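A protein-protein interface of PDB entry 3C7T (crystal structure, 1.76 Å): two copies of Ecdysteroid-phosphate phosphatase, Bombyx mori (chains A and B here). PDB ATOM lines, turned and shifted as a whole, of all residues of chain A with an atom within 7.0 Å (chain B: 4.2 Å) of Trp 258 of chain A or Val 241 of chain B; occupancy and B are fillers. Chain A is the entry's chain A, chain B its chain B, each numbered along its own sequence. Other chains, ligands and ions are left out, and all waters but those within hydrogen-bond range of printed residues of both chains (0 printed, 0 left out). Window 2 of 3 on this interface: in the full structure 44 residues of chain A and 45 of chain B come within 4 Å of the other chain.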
ATOM      1  N   PHE A 256       3.723 -12.068 -26.025  1.00  0.00           N
ATOM      2  CA  PHE A 256       3.734 -11.324 -24.770  1.00  0.00           C
ATOM      3  C   PHE A 256       2.467 -10.470 -24.625  1.00  0.00           C
ATOM      4  O   PHE A 256       2.006  -9.881 -25.617  1.00  0.00           O
ATOM      5  CB  PHE A 256       4.963 -10.411 -24.702  1.00  0.00           C
ATOM      6  CG  PHE A 256       5.047  -9.605 -23.446  1.00  0.00           C
ATOM      7  CD1 PHE A 256       5.042 -10.234 -22.211  1.00  0.00           C
ATOM      8  CD2 PHE A 256       5.174  -8.231 -23.501  1.00  0.00           C
ATOM      9  CE1 PHE A 256       5.133  -9.517 -21.061  1.00  0.00           C
ATOM     10  CE2 PHE A 256       5.283  -7.493 -22.342  1.00  0.00           C
ATOM     11  CZ  PHE A 256       5.247  -8.127 -21.117  1.00  0.00           C
ATOM     12  N   ASP A 257       1.936 -10.373 -23.404  1.00  0.00           N
ATOM     13  CA  ASP A 257       0.775  -9.497 -23.127  1.00  0.00           C
ATOM     14  C   ASP A 257       1.216  -8.423 -22.119  1.00  0.00           C
ATOM     15  O   ASP A 257       1.394  -8.708 -20.926  1.00  0.00           O
ATOM     16  CB  ASP A 257      -0.406 -10.317 -22.584  1.00  0.00           C
ATOM     17  CG  ASP A 257      -1.647  -9.454 -22.248  1.00  0.00           C
ATOM     18  OD1 ASP A 257      -1.634  -8.209 -22.425  1.00  0.00           O
ATOM     19  OD2 ASP A 257      -2.663 -10.050 -21.788  1.00  0.00           O
ATOM     20  N   TRP A 258       1.444  -7.208 -22.606  1.00  0.00           N
ATOM     21  CA  TRP A 258       2.044  -6.153 -21.777  1.00  0.00           C
ATOM     22  C   TRP A 258       1.258  -5.855 -20.501  1.00  0.00           C
ATOM     23  O   TRP A 258       1.811  -5.331 -19.514  1.00  0.00           O
ATOM     24  CB  TRP A 258       2.232  -4.864 -22.583  1.00  0.00           C
ATOM     25  CG  TRP A 258       0.944  -4.222 -23.024  1.00  0.00           C
ATOM     26  CD1 TRP A 258       0.287  -4.437 -24.205  1.00  0.00           C
ATOM     27  CD2 TRP A 258       0.164  -3.255 -22.299  1.00  0.00           C
ATOM     28  NE1 TRP A 258      -0.855  -3.677 -24.250  1.00  0.00           N
ATOM     29  CE2 TRP A 258      -0.957  -2.942 -23.096  1.00  0.00           C
ATOM     30  CE3 TRP A 258       0.302  -2.632 -21.045  1.00  0.00           C
ATOM     31  CZ2 TRP A 258      -1.951  -2.021 -22.686  1.00  0.00           C
ATOM     32  CZ3 TRP A 258      -0.696  -1.702 -20.626  1.00  0.00           C
ATOM     33  CH2 TRP A 258      -1.797  -1.408 -21.456  1.00  0.00           C
ATOM     34  N   ARG A 259      -0.031  -6.195 -20.525  1.00  0.00           N
ATOM     35  CA  ARG A 259      -0.929  -5.906 -19.385  1.00  0.00           C
ATOM     36  C   ARG A 259      -0.541  -6.662 -18.105  1.00  0.00           C
ATOM     37  O   ARG A 259      -0.964  -6.288 -16.997  1.00  0.00           O
ATOM     38  CB  ARG A 259      -2.391  -6.163 -19.777  1.00  0.00           C
ATOM     39  CG  ARG A 259      -2.795  -5.348 -21.007  1.00  0.00           C
ATOM     40  CD  ARG A 259      -4.192  -5.672 -21.561  1.00  0.00           C
ATOM     41  NE  ARG A 259      -4.390  -4.994 -22.857  1.00  0.00           N
ATOM     42  CZ  ARG A 259      -4.912  -3.770 -23.020  1.00  0.00           C
ATOM     43  NH1 ARG A 259      -5.311  -3.054 -21.970  1.00  0.00           N
ATOM     44  NH2 ARG A 259      -5.029  -3.251 -24.241  1.00  0.00           N
ATOM     45  N   ILE A 260       0.274  -7.709 -18.225  1.00  0.00           N
ATOM     46  CA  ILE A 260       0.774  -8.381 -17.014  1.00  0.00           C
ATOM     47  C   ILE A 260       1.750  -7.484 -16.228  1.00  0.00           C
ATOM     48  O   ILE A 260       2.062  -7.745 -15.055  1.00  0.00           O
ATOM     49  CB  ILE A 260       1.425  -9.749 -17.320  1.00  0.00           C
ATOM     50  CG1 ILE A 260       2.738  -9.576 -18.086  1.00  0.00           C
ATOM     51  CG2 ILE A 260       0.438 -10.657 -18.077  1.00  0.00           C
ATOM     52  CD1 ILE A 260       3.970  -9.823 -17.257  1.00  0.00           C
ATOM     53  N   LEU A 261       2.246  -6.434 -16.890  1.00  0.00           N
ATOM     54  CA  LEU A 261       3.147  -5.490 -16.231  1.00  0.00           C
ATOM     55  C   LEU A 261       2.427  -4.589 -15.242  1.00  0.00           C
ATOM     56  O   LEU A 261       3.052  -4.015 -14.354  1.00  0.00           O
ATOM     57  CB  LEU A 261       3.922  -4.657 -17.259  1.00  0.00           C
ATOM     58  CG  LEU A 261       4.908  -5.444 -18.129  1.00  0.00           C
ATOM     59  CD1 LEU A 261       5.477  -4.522 -19.189  1.00  0.00           C
ATOM     60  CD2 LEU A 261       6.021  -6.049 -17.288  1.00  0.00           C
ATOM     61  N   ILE A 262       1.110  -4.454 -15.388  1.00  0.00           N
ATOM     62  CA  ILE A 262       0.358  -3.602 -14.459  1.00  0.00           C
ATOM     63  C   ILE A 262      -0.241  -4.387 -13.294  1.00  0.00           C
ATOM     64  O   ILE A 262       0.447  -4.632 -12.295  1.00  0.00           O
ATOM     65  CB  ILE A 262      -0.696  -2.722 -15.171  1.00  0.00           C
ATOM     66  CG1 ILE A 262      -1.355  -3.478 -16.321  1.00  0.00           C
ATOM     67  CG2 ILE A 262      -0.035  -1.466 -15.690  1.00  0.00           C
ATOM     68  CD1 ILE A 262      -2.279  -2.658 -17.201  1.00  0.00           C
ATOM     69  N   TRP B   6       8.996   8.054 -24.381  1.00  0.00           N
ATOM     70  CA  TRP B   6       8.928   6.614 -24.172  1.00  0.00           C
ATOM     71  C   TRP B   6      10.173   6.086 -23.462  1.00  0.00           C
ATOM     72  O   TRP B   6      11.305   6.533 -23.718  1.00  0.00           O
ATOM     73  CB  TRP B   6       8.879   5.901 -25.518  1.00  0.00           C
ATOM     74  CG  TRP B   6       7.684   6.148 -26.383  1.00  0.00           C
ATOM     75  CD1 TRP B   6       7.576   7.074 -27.383  1.00  0.00           C
ATOM     76  CD2 TRP B   6       6.472   5.391 -26.403  1.00  0.00           C
ATOM     77  NE1 TRP B   6       6.358   6.948 -28.019  1.00  0.00           N
ATOM     78  CE2 TRP B   6       5.658   5.934 -27.425  1.00  0.00           C
ATOM     79  CE3 TRP B   6       5.986   4.307 -25.650  1.00  0.00           C
ATOM     80  CZ2 TRP B   6       4.395   5.430 -27.712  1.00  0.00           C
ATOM     81  CZ3 TRP B   6       4.721   3.808 -25.936  1.00  0.00           C
ATOM     82  CH2 TRP B   6       3.940   4.378 -26.953  1.00  0.00           C
ATOM     83  N   ALA B 232       6.593  -1.083 -22.244  1.00  0.00           N
ATOM     84  CA  ALA B 232       6.658   0.340 -22.548  1.00  0.00           C
ATOM     85  C   ALA B 232       6.038   1.187 -21.438  1.00  0.00           C
ATOM     86  O   ALA B 232       5.040   0.786 -20.826  1.00  0.00           O
ATOM     87  CB  ALA B 232       5.957   0.612 -23.843  1.00  0.00           C
ATOM     88  N   ARG B 234       5.297   5.605 -20.630  1.00  0.00           N
ATOM     89  CA  ARG B 234       5.387   6.986 -21.083  1.00  0.00           C
ATOM     90  C   ARG B 234       5.291   7.900 -19.881  1.00  0.00           C
ATOM     91  O   ARG B 234       4.633   7.560 -18.885  1.00  0.00           O
ATOM     92  CB  ARG B 234       4.297   7.325 -22.099  1.00  0.00           C
ATOM     93  CG  ARG B 234       4.589   6.785 -23.484  1.00  0.00           C
ATOM     94  CD  ARG B 234       3.641   7.365 -24.504  1.00  0.00           C
ATOM     95  NE  ARG B 234       4.102   8.661 -24.999  1.00  0.00           N
ATOM     96  CZ  ARG B 234       3.719   9.188 -26.159  1.00  0.00           C
ATOM     97  NH1 ARG B 234       2.856   8.532 -26.937  1.00  0.00           N
ATOM     98  NH2 ARG B 234       4.189  10.372 -26.549  1.00  0.00           N
ATOM     99  N   ASP B 239       3.890   5.846 -16.629  1.00  0.00           N
ATOM    100  CA  ASP B 239       2.731   4.975 -16.709  1.00  0.00           C
ATOM    101  C   ASP B 239       3.012   3.865 -17.700  1.00  0.00           C
ATOM    102  O   ASP B 239       3.597   4.115 -18.748  1.00  0.00           O
ATOM    103  CB  ASP B 239       1.507   5.766 -17.182  1.00  0.00           C
ATOM    104  CG  ASP B 239       1.018   6.775 -16.142  1.00  0.00           C
ATOM    105  OD1 ASP B 239       1.050   6.464 -14.925  1.00  0.00           O
ATOM    106  OD2 ASP B 239       0.585   7.879 -16.542  1.00  0.00           O
ATOM    107  N   VAL B 240       2.596   2.648 -17.353  1.00  0.00           N
ATOM    108  CA  VAL B 240       2.660   1.495 -18.241  1.00  0.00           C
ATOM    109  C   VAL B 240       1.603   1.618 -19.329  1.00  0.00           C
ATOM    110  O   VAL B 240       0.412   1.810 -19.051  1.00  0.00           O
ATOM    111  CB  VAL B 240       2.435   0.198 -17.462  1.00  0.00           C
ATOM    112  CG1 VAL B 240       2.468  -1.012 -18.392  1.00  0.00           C
ATOM    113  CG2 VAL B 240       3.476   0.061 -16.361  1.00  0.00           C
ATOM    114  N   VAL B 241       2.040   1.532 -20.575  1.00  0.00           N
ATOM    115  CA  VAL B 241       1.146   1.715 -21.700  1.00  0.00           C
ATOM    116  C   VAL B 241       1.405   0.628 -22.724  1.00  0.00           C
ATOM    117  O   VAL B 241       2.445  -0.022 -22.706  1.00  0.00           O
ATOM    118  CB  VAL B 241       1.314   3.137 -22.365  1.00  0.00           C
ATOM    119  CG1 VAL B 241       1.059   4.298 -21.344  1.00  0.00           C
ATOM    120  CG2 VAL B 241       2.694   3.286 -22.999  1.00  0.00           C
ATOM    121  N   SER B 242       0.468   0.451 -23.646  1.00  0.00           N
ATOM    122  CA  SER B 242       0.697  -0.397 -24.804  1.00  0.00           C
ATOM    123  C   SER B 242       1.899   0.106 -25.626  1.00  0.00           C
ATOM    124  O   SER B 242       1.936   1.279 -26.028  1.00  0.00           O
ATOM    125  CB  SER B 242      -0.533  -0.404 -25.689  1.00  0.00           C
ATOM    126  OG  SER B 242      -0.288  -1.176 -26.850  1.00  0.00           O
ATOM    127  N   PRO B 243       2.886  -0.779 -25.889  1.00  0.00           N
ATOM    128  CA  PRO B 243       3.972  -0.373 -26.771  1.00  0.00           C
ATOM    129  C   PRO B 243       3.426   0.003 -28.160  1.00  0.00           C
ATOM    130  O   PRO B 243       2.298  -0.381 -28.485  1.00  0.00           O
ATOM    131  CB  PRO B 243       4.840  -1.641 -26.861  1.00  0.00           C
ATOM    132  CG  PRO B 243       4.494  -2.423 -25.690  1.00  0.00           C
ATOM    133  CD  PRO B 243       3.071  -2.159 -25.394  1.00  0.00           C
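Among the printed residues, pairs that only touch across the chains: Trp 258 of chain A with Val 240 of chain B (3.8 Å), Trp 258 of chain A with Val 241 of chain B (3.8 Å), Trp 258 of chain A with Ser 242 of chain B (3.5 Å), Trp 258 of chain A with Pro 243 of chain B (3.8 Å) and Ile 262 of chain A with Val 240 of chain B (3.5 Å).
No position is printed for both chains.
Of the 5 pairs that touch across the chains among the printed residues, none has its exchanged pair printed and touching as well.
Hydrophobic or aromatic side chains of chain B within 4 Å of the printed part of chain A: Val 240 and Pro 243.
Of the 7 printed residues of chain A, 2 touch a printed residue of chain B.
Along chain A the printed residues that touch a printed residue of chain B span positions 258 to 262.
Among the printed residues, 5 pairs touch across the chains.
The backbone carbonyl oxygen (O) of Ala 232 of chain B is in hydrogen-bond range of the backbone NH (N) of Val 241 of chain B (3.1 Å).
Asp 257 of chain A touches none of the printed residues of chain B.
Of the printed residues of chain B, Trp 258 of chain A touches Val 240 (3.8 Å), Val 241 (3.8 Å), Ser 242 (3.5 Å) and Pro 243 (3.8 Å).
Of the printed residues of chain A, Val 240 of chain B touches Trp 258 (3.8 Å) and Ile 262 (3.5 Å).
Val 241 of chain B touches one residue of chain A.
Printed residues of chain A within 4 Å of Ser 242 of chain B: Trp 258 (3.5 Å).
The nearest printed residue of chain B that does not touch Trp 258 of chain A is Ala 232 of chain B (5.8 Å).
The nearest printed residue of chain A that does not touch Pro 243 of chain B is Phe 256 of chain A (6.1 Å).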
